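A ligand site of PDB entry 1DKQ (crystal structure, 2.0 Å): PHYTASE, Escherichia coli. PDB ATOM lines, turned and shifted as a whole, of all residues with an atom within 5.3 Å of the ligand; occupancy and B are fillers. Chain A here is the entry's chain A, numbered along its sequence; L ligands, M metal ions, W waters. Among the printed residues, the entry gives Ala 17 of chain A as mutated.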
ATOM      1  N   ARG A  16      -2.552  23.476  23.357  1.00  0.00           N
ATOM      2  CA  ARG A  16      -3.889  23.471  22.810  1.00  0.00           C
ATOM      3  C   ARG A  16      -4.144  24.951  22.572  1.00  0.00           C
ATOM      4  O   ARG A  16      -3.501  25.801  23.216  1.00  0.00           O
ATOM      5  CB  ARG A  16      -4.900  22.944  23.820  1.00  0.00           C
ATOM      6  CG  ARG A  16      -6.332  23.183  23.368  1.00  0.00           C
ATOM      7  CD  ARG A  16      -7.358  22.713  24.366  1.00  0.00           C
ATOM      8  NE  ARG A  16      -8.692  22.899  23.813  1.00  0.00           N
ATOM      9  CZ  ARG A  16      -9.802  22.966  24.541  1.00  0.00           C
ATOM     10  NH1 ARG A  16      -9.753  22.855  25.865  1.00  0.00           N
ATOM     11  NH2 ARG A  16     -10.973  23.166  23.939  1.00  0.00           N
ATOM     12  N   ALA A  17      -5.055  25.268  21.663  1.00  0.00           N
ATOM     13  CA  ALA A  17      -5.381  26.661  21.408  1.00  0.00           C
ATOM     14  C   ALA A  17      -6.010  27.199  22.697  1.00  0.00           C
ATOM     15  O   ALA A  17      -6.417  26.426  23.563  1.00  0.00           O
ATOM     16  CB  ALA A  17      -6.376  26.780  20.254  1.00  0.00           C
ATOM     17  N   ARG A  20     -11.718  30.186  23.358  1.00  0.00           N
ATOM     18  CA  ARG A  20     -12.392  30.530  22.109  1.00  0.00           C
ATOM     19  C   ARG A  20     -13.893  30.448  22.341  1.00  0.00           C
ATOM     20  O   ARG A  20     -14.344  29.919  23.366  1.00  0.00           O
ATOM     21  CB  ARG A  20     -12.025  29.500  21.033  1.00  0.00           C
ATOM     22  CG  ARG A  20     -12.377  28.075  21.478  1.00  0.00           C
ATOM     23  CD  ARG A  20     -12.421  27.088  20.312  1.00  0.00           C
ATOM     24  NE  ARG A  20     -12.563  25.699  20.752  1.00  0.00           N
ATOM     25  CZ  ARG A  20     -13.677  25.167  21.255  1.00  0.00           C
ATOM     26  NH1 ARG A  20     -13.692  23.889  21.624  1.00  0.00           N
ATOM     27  NH2 ARG A  20     -14.778  25.906  21.383  1.00  0.00           N
ATOM     28  N   THR A  23     -17.597  26.202  18.982  1.00  0.00           N
ATOM     29  CA  THR A  23     -17.451  25.989  17.545  1.00  0.00           C
ATOM     30  C   THR A  23     -18.779  25.965  16.803  1.00  0.00           C
ATOM     31  O   THR A  23     -18.814  26.189  15.592  1.00  0.00           O
ATOM     32  CB  THR A  23     -16.702  24.673  17.243  1.00  0.00           C
ATOM     33  OG1 THR A  23     -17.413  23.568  17.799  1.00  0.00           O
ATOM     34  CG2 THR A  23     -15.290  24.716  17.828  1.00  0.00           C
ATOM     35  N   LYS A  24     -19.871  25.701  17.505  1.00  0.00           N
ATOM     36  CA  LYS A  24     -21.167  25.663  16.829  1.00  0.00           C
ATOM     37  C   LYS A  24     -22.332  26.138  17.683  1.00  0.00           C
ATOM     38  O   LYS A  24     -22.218  26.284  18.897  1.00  0.00           O
ATOM     39  CB  LYS A  24     -21.444  24.244  16.309  1.00  0.00           C
ATOM     40  CG  LYS A  24     -21.364  23.174  17.366  1.00  0.00           C
ATOM     41  CD  LYS A  24     -21.263  21.790  16.747  1.00  0.00           C
ATOM     42  CE  LYS A  24     -20.013  21.666  15.875  1.00  0.00           C
ATOM     43  NZ  LYS A  24     -19.867  20.311  15.292  1.00  0.00           N
ATOM     44  N   ASP A  90      -6.045  26.693  11.521  1.00  0.00           N
ATOM     45  CA  ASP A  90      -7.197  27.375  12.122  1.00  0.00           C
ATOM     46  C   ASP A  90      -6.891  28.789  12.631  1.00  0.00           C
ATOM     47  O   ASP A  90      -5.749  29.100  12.982  1.00  0.00           O
ATOM     48  CB  ASP A  90      -7.779  26.551  13.275  1.00  0.00           C
ATOM     49  CG  ASP A  90      -8.289  25.172  12.829  1.00  0.00           C
ATOM     50  OD1 ASP A  90      -8.482  24.966  11.613  1.00  0.00           O
ATOM     51  OD2 ASP A  90      -8.511  24.313  13.700  1.00  0.00           O
ATOM     52  N   ARG A  92      -7.947  30.117  15.441  1.00  0.00           N
ATOM     53  CA  ARG A  92      -7.581  30.051  16.850  1.00  0.00           C
ATOM     54  C   ARG A  92      -6.174  29.523  17.153  1.00  0.00           C
ATOM     55  O   ARG A  92      -5.563  29.958  18.129  1.00  0.00           O
ATOM     56  CB  ARG A  92      -8.629  29.249  17.642  1.00  0.00           C
ATOM     57  CG  ARG A  92      -8.800  27.783  17.268  1.00  0.00           C
ATOM     58  CD  ARG A  92      -9.724  27.124  18.285  1.00  0.00           C
ATOM     59  NE  ARG A  92     -10.072  25.743  17.963  1.00  0.00           N
ATOM     60  CZ  ARG A  92     -10.906  25.378  17.002  1.00  0.00           C
ATOM     61  NH1 ARG A  92     -11.501  26.292  16.237  1.00  0.00           N
ATOM     62  NH2 ARG A  92     -11.166  24.090  16.802  1.00  0.00           N
ATOM     63  N   LYS A 129      -7.983  12.458   9.062  1.00  0.00           N
ATOM     64  CA  LYS A 129      -8.869  13.376   8.374  1.00  0.00           C
ATOM     65  C   LYS A 129      -8.459  13.653   6.924  1.00  0.00           C
ATOM     66  O   LYS A 129      -9.317  13.788   6.049  1.00  0.00           O
ATOM     67  CB  LYS A 129      -8.950  14.688   9.160  1.00  0.00           C
ATOM     68  CG  LYS A 129      -9.911  15.715   8.600  1.00  0.00           C
ATOM     69  CD  LYS A 129     -10.238  16.797   9.619  1.00  0.00           C
ATOM     70  CE  LYS A 129      -9.024  17.598  10.025  1.00  0.00           C
ATOM     71  NZ  LYS A 129      -9.379  18.673  10.999  1.00  0.00           N
ATOM     72  N   SER A 212     -21.516  12.981  23.325  1.00  0.00           N
ATOM     73  CA  SER A 212     -20.827  14.066  22.636  1.00  0.00           C
ATOM     74  C   SER A 212     -21.436  15.429  22.930  1.00  0.00           C
ATOM     75  O   SER A 212     -20.724  16.437  22.982  1.00  0.00           O
ATOM     76  CB  SER A 212     -20.822  13.813  21.129  1.00  0.00           C
ATOM     77  OG  SER A 212     -22.141  13.610  20.650  1.00  0.00           O
ATOM     78  N   SER A 215     -20.119  16.415  26.344  1.00  0.00           N
ATOM     79  CA  SER A 215     -18.697  16.747  26.312  1.00  0.00           C
ATOM     80  C   SER A 215     -18.540  18.173  25.791  1.00  0.00           C
ATOM     81  O   SER A 215     -17.744  18.952  26.302  1.00  0.00           O
ATOM     82  CB  SER A 215     -17.913  15.765  25.433  1.00  0.00           C
ATOM     83  OG  SER A 215     -16.551  16.138  25.353  1.00  0.00           O
ATOM     84  N   MET A 216     -19.318  18.504  24.767  1.00  0.00           N
ATOM     85  CA  MET A 216     -19.271  19.842  24.178  1.00  0.00           C
ATOM     86  C   MET A 216     -19.867  20.923  25.106  1.00  0.00           C
ATOM     87  O   MET A 216     -19.272  21.981  25.321  1.00  0.00           O
ATOM     88  CB  MET A 216     -20.027  19.837  22.848  1.00  0.00           C
ATOM     89  CG  MET A 216     -20.022  21.175  22.123  1.00  0.00           C
ATOM     90  SD  MET A 216     -21.244  21.203  20.805  1.00  0.00           S
ATOM     91  CE  MET A 216     -20.554  20.022  19.682  1.00  0.00           C
ATOM     92  N   GLU A 219     -17.717  21.700  28.181  1.00  0.00           N
ATOM     93  CA  GLU A 219     -16.530  22.424  27.788  1.00  0.00           C
ATOM     94  C   GLU A 219     -16.936  23.885  27.547  1.00  0.00           C
ATOM     95  O   GLU A 219     -16.171  24.799  27.841  1.00  0.00           O
ATOM     96  CB  GLU A 219     -15.938  21.829  26.506  1.00  0.00           C
ATOM     97  CG  GLU A 219     -14.799  22.666  25.907  1.00  0.00           C
ATOM     98  CD  GLU A 219     -13.552  22.721  26.784  1.00  0.00           C
ATOM     99  OE1 GLU A 219     -12.642  23.513  26.444  1.00  0.00           O
ATOM    100  OE2 GLU A 219     -13.461  21.985  27.790  1.00  0.00           O
ATOM    101  N   HIS A 250     -16.737  15.525  29.817  1.00  0.00           N
ATOM    102  CA  HIS A 250     -15.864  15.914  28.737  1.00  0.00           C
ATOM    103  C   HIS A 250     -14.635  14.994  28.730  1.00  0.00           C
ATOM    104  O   HIS A 250     -14.277  14.430  27.701  1.00  0.00           O
ATOM    105  CB  HIS A 250     -15.457  17.362  28.942  1.00  0.00           C
ATOM    106  CG  HIS A 250     -14.590  17.898  27.856  1.00  0.00           C
ATOM    107  ND1 HIS A 250     -15.044  18.102  26.562  1.00  0.00           N
ATOM    108  CD2 HIS A 250     -13.285  18.255  27.857  1.00  0.00           C
ATOM    109  CE1 HIS A 250     -14.045  18.554  25.827  1.00  0.00           C
ATOM    110  NE2 HIS A 250     -12.971  18.654  26.582  1.00  0.00           N
ATOM    111  N   PHE A 254     -13.137  11.998  25.839  1.00  0.00           N
ATOM    112  CA  PHE A 254     -11.780  12.014  25.336  1.00  0.00           C
ATOM    113  C   PHE A 254     -11.037  10.727  25.688  1.00  0.00           C
ATOM    114  O   PHE A 254     -10.191  10.255  24.930  1.00  0.00           O
ATOM    115  CB  PHE A 254     -11.019  13.245  25.855  1.00  0.00           C
ATOM    116  CG  PHE A 254     -11.149  14.453  24.965  1.00  0.00           C
ATOM    117  CD1 PHE A 254     -12.391  15.007  24.685  1.00  0.00           C
ATOM    118  CD2 PHE A 254     -10.018  15.022  24.380  1.00  0.00           C
ATOM    119  CE1 PHE A 254     -12.519  16.102  23.837  1.00  0.00           C
ATOM    120  CE2 PHE A 254     -10.136  16.116  23.530  1.00  0.00           C
ATOM    121  CZ  PHE A 254     -11.388  16.656  23.252  1.00  0.00           C
ATOM    122  N   ARG A 267      -3.297   8.834  15.110  1.00  0.00           N
ATOM    123  CA  ARG A 267      -3.605  10.267  15.096  1.00  0.00           C
ATOM    124  C   ARG A 267      -2.470  11.172  15.537  1.00  0.00           C
ATOM    125  O   ARG A 267      -2.356  12.313  15.065  1.00  0.00           O
ATOM    126  CB  ARG A 267      -4.864  10.540  15.949  1.00  0.00           C
ATOM    127  CG  ARG A 267      -5.680  11.755  15.509  1.00  0.00           C
ATOM    128  CD  ARG A 267      -7.107  11.693  16.066  1.00  0.00           C
ATOM    129  NE  ARG A 267      -7.937  12.829  15.649  1.00  0.00           N
ATOM    130  CZ  ARG A 267      -7.774  14.083  16.051  1.00  0.00           C
ATOM    131  NH1 ARG A 267      -6.801  14.397  16.917  1.00  0.00           N
ATOM    132  NH2 ARG A 267      -8.572  15.036  15.600  1.00  0.00           N
ATOM    133  N   GLY A 302      -1.687  23.399  18.670  1.00  0.00           N
ATOM    134  CA  GLY A 302      -2.609  22.389  18.208  1.00  0.00           C
ATOM    135  C   GLY A 302      -3.953  22.406  18.917  1.00  0.00           C
ATOM    136  O   GLY A 302      -4.479  23.460  19.281  1.00  0.00           O
ATOM    137  N   HIS A 303      -4.508  21.217  19.167  1.00  0.00           N
ATOM    138  CA  HIS A 303      -5.824  21.108  19.770  1.00  0.00           C
ATOM    139  C   HIS A 303      -5.876  20.153  20.971  1.00  0.00           C
ATOM    140  O   HIS A 303      -4.902  19.448  21.252  1.00  0.00           O
ATOM    141  CB  HIS A 303      -6.814  20.626  18.706  1.00  0.00           C
ATOM    142  CG  HIS A 303      -6.767  21.412  17.433  1.00  0.00           C
ATOM    143  ND1 HIS A 303      -7.459  22.593  17.252  1.00  0.00           N
ATOM    144  CD2 HIS A 303      -6.120  21.178  16.265  1.00  0.00           C
ATOM    145  CE1 HIS A 303      -7.239  23.045  16.035  1.00  0.00           C
ATOM    146  NE2 HIS A 303      -6.430  22.209  15.404  1.00  0.00           N
ATOM    147  N   ASP A 304      -7.009  20.107  21.659  1.00  0.00           N
ATOM    148  CA  ASP A 304      -7.102  19.221  22.809  1.00  0.00           C
ATOM    149  C   ASP A 304      -6.970  17.744  22.422  1.00  0.00           C
ATOM    150  O   ASP A 304      -6.345  16.972  23.154  1.00  0.00           O
ATOM    151  CB  ASP A 304      -8.378  19.473  23.616  1.00  0.00           C
ATOM    152  CG  ASP A 304      -9.613  19.489  22.766  1.00  0.00           C
ATOM    153  OD1 ASP A 304     -10.688  19.885  23.288  1.00  0.00           O
ATOM    154  OD2 ASP A 304      -9.541  19.115  21.584  1.00  0.00           O
ATOM    155  N   THR A 305      -7.520  17.355  21.278  1.00  0.00           N
ATOM    156  CA  THR A 305      -7.418  15.955  20.846  1.00  0.00           C
ATOM    157  C   THR A 305      -5.950  15.562  20.624  1.00  0.00           C
ATOM    158  O   THR A 305      -5.561  14.427  20.827  1.00  0.00           O
ATOM    159  CB  THR A 305      -8.212  15.715  19.543  1.00  0.00           C
ATOM    160  OG1 THR A 305      -7.674  16.530  18.491  1.00  0.00           O
ATOM    161  CG2 THR A 305      -9.690  16.037  19.752  1.00  0.00           C
ATOM    162  N   ASN A 306      -5.134  16.522  20.186  1.00  0.00           N
ATOM    163  CA  ASN A 306      -3.709  16.255  19.972  1.00  0.00           C
ATOM    164  C   ASN A 306      -3.042  15.917  21.301  1.00  0.00           C
ATOM    165  O   ASN A 306      -2.263  14.973  21.390  1.00  0.00           O
ATOM    166  CB  ASN A 306      -3.031  17.494  19.372  1.00  0.00           C
ATOM    167  CG  ASN A 306      -3.525  17.824  17.986  1.00  0.00           C
ATOM    168  OD1 ASN A 306      -3.809  18.985  17.687  1.00  0.00           O
ATOM    169  ND2 ASN A 306      -3.621  16.818  17.115  1.00  0.00           N
HETATM  170  C1  LIG L   1     -12.992  21.055  16.873  1.00  0.00           C
HETATM  171  C2  LIG L   1     -11.701  20.892  17.720  1.00  0.00           C
HETATM  172  C3  LIG L   1     -11.916  21.457  19.184  1.00  0.00           C
HETATM  173  C4  LIG L   1     -13.121  20.714  19.895  1.00  0.00           C
HETATM  174  C5  LIG L   1     -14.395  20.737  19.001  1.00  0.00           C
HETATM  175  C6  LIG L   1     -14.128  20.259  17.557  1.00  0.00           C
HETATM  176  O1  LIG L   1     -12.777  20.546  15.538  1.00  0.00           O
HETATM  177  P1  LIG L   1     -12.187  21.484  14.399  1.00  0.00           P
HETATM  178  O2  LIG L   1     -12.855  22.931  14.544  1.00  0.00           O
HETATM  179  O3  LIG L   1     -12.517  20.885  13.067  1.00  0.00           O
HETATM  180  O4  LIG L   1     -10.601  21.664  14.526  1.00  0.00           O
HETATM  181  O5  LIG L   1     -11.362  19.495  17.808  1.00  0.00           O
HETATM  182  P2  LIG L   1      -9.958  18.919  17.280  1.00  0.00           P
HETATM  183  O6  LIG L   1     -10.148  17.483  16.609  1.00  0.00           O
HETATM  184  O7  LIG L   1      -9.334  19.829  16.279  1.00  0.00           O
HETATM  185  O8  LIG L   1      -8.986  18.741  18.524  1.00  0.00           O
HETATM  186  O9  LIG L   1     -10.722  21.299  19.940  1.00  0.00           O
HETATM  187  P3  LIG L   1      -9.871  22.634  20.286  1.00  0.00           P
HETATM  188  O10 LIG L   1     -10.734  23.615  20.992  1.00  0.00           O
HETATM  189  O11 LIG L   1      -9.335  23.296  18.947  1.00  0.00           O
HETATM  190  O12 LIG L   1      -8.652  22.255  21.202  1.00  0.00           O
HETATM  191  O13 LIG L   1     -13.460  21.348  21.122  1.00  0.00           O
HETATM  192  P4  LIG L   1     -13.901  20.435  22.372  1.00  0.00           P
HETATM  193  O14 LIG L   1     -13.064  20.834  23.541  1.00  0.00           O
HETATM  194  O15 LIG L   1     -13.753  18.872  22.126  1.00  0.00           O
HETATM  195  O16 LIG L   1     -15.429  20.754  22.705  1.00  0.00           O
HETATM  196  O17 LIG L   1     -15.433  19.910  19.534  1.00  0.00           O
HETATM  197  P5  LIG L   1     -16.905  20.522  19.722  1.00  0.00           P
HETATM  198  O18 LIG L   1     -16.860  22.010  19.707  1.00  0.00           O
HETATM  199  O19 LIG L   1     -17.839  19.993  18.554  1.00  0.00           O
HETATM  200  O20 LIG L   1     -17.480  20.049  21.118  1.00  0.00           O
HETATM  201  O21 LIG L   1     -15.369  20.372  16.823  1.00  0.00           O
HETATM  202  P6  LIG L   1     -15.916  19.167  15.940  1.00  0.00           P
HETATM  203  O22 LIG L   1     -16.936  19.737  14.864  1.00  0.00           O
HETATM  204  O23 LIG L   1     -16.680  18.112  16.864  1.00  0.00           O
HETATM  205  O24 LIG L   1     -14.791  18.491  15.236  1.00  0.00           O
HETATM  206 HG    HG M   1     -11.221  20.466  26.152  1.00  0.00          HG
HETATM  207 HG    HG M   2     -10.318  19.047  26.771  1.00  0.00          HG
HETATM  208  O   HOH W   1      -9.245  26.114  21.712  1.00  0.00           O
HETATM  209  O   HOH W   2     -16.872  23.004  23.369  1.00  0.00           O
HETATM  210  O   HOH W   3      -6.788  18.350  15.157  1.00  0.00           O
HETATM  211  O   HOH W   4     -13.963  25.702  14.518  1.00  0.00           O
HETATM  212  O   HOH W   5     -16.389  17.761  22.934  1.00  0.00           O
HETATM  213  O   HOH W   6     -17.385  24.127  21.237  1.00  0.00           O
HETATM  214  O   HOH W   7      -8.114  21.713  12.640  1.00  0.00           O
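The side-chain hydroxyl of Thr 23 sits at hydrogen-bond distance from an oxygen (O18) of the ligand (2.5 Å).
NH2 of Arg 267 lies within salt-bridge range of O6 of the ligand (3.1 Å).
NZ of Lys 24 is in salt-bridge range of O22 of the ligand (3.0 Å).
The backbone NH of Thr 305 sits close to an oxygen (O8) of the ligand, 3.4 Å away.
The guanidinium group (NE) of Arg 92 is in salt-bridge range of an oxygen (O11) of the ligand, at 2.7 Å.
An oxygen (O11) of the ligand sits at hydrogen-bond distance from a ring nitrogen (ND1) of His 303 (2.6 Å).
O12 of the ligand is in hydrogen-bond range of N of Asp 304.
An oxygen (O8) of the ligand is in hydrogen-bond range of the side-chain hydroxyl of Thr 305, at 2.6 Å.
The guanidinium group (NE) of Arg 16 lies within salt-bridge range of an oxygen (O12) of the ligand (2.7 Å).
OD1 of Asp 304 lies close to O14 of the ligand (2.6 Å).
The guanidinium group of Arg 20 lies within salt-bridge range of an oxygen (O10) of the ligand (2.8 Å).
The guanidinium group (NH1) of Arg 267 is in hydrogen-bond range of the side-chain hydroxyl (OG1) of Thr 305, 2.8 Å away.
A ring nitrogen (ND1) of His 250 lies within hydrogen-bond range of the side-chain hydroxyl of Ser 215 (2.8 Å).
The side-chain amide oxygen (OD1) of Asn 306 is in hydrogen-bond range of the backbone NH (N) of His 303, at 2.8 Å.
The side-chain carboxylate (OD1) of Asp 304 is in salt-bridge range of the guanidinium group (NH2) of Arg 16 (3.4 Å).
OD2 of Asp 90 sits close to NE2 of His 303 (3.4 Å).
NH1 of Arg 16 lies within salt-bridge range of OE1 of Glu 219, at 3.0 Å.
O4 of the ligand sits close to OD2 of Asp 90, 3.5 Å away.
Met 216 touches the ligand.
Glu 219 touches the ligand (CG to O14, 3.5 Å).
His 250 touches the ligand (CE1 to O14, 3.4 Å).
CZ of Phe 254 touches O15 of the ligand (3.4 Å).
Hydrophobic or aromatic side chains within 4 Å of the ligand: Met 216, His 250, Phe 254 and His 303.
Of the 20 residues printed, 14 come within 4 Å of the ligand.
The nearest printed residue that does not touch the ligand is Lys 129 (4.4 Å).
Water W6 lies within hydrogen-bond range of O18 of the ligand (2.7 Å), N of Thr 23 (3.1 Å) and NH2 of Arg 20 (3.2 Å).
Water W2 bridges O16 of the ligand (2.8 Å) and O of Met 216 (3.3 Å).
Water W5 lies within hydrogen-bond range of the side-chain hydroxyl of Ser 215 (2.9 Å) and an oxygen (O15) of the ligand (3.0 Å).
Water W4 bridges O2 of the ligand and NH1 of Arg 92.
Water W1 lies within hydrogen-bond range of an oxygen (O10) of the ligand, the backbone carbonyl oxygen of Ala 17 and the guanidinium group of Arg 20.
Water W7 lies within hydrogen-bond range of the side-chain carboxylate (OD2) of Asp 90 (2.8 Å), an oxygen (O4) of the ligand (3.1 Å) and a ring nitrogen (NE2) of His 303 (3.3 Å).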
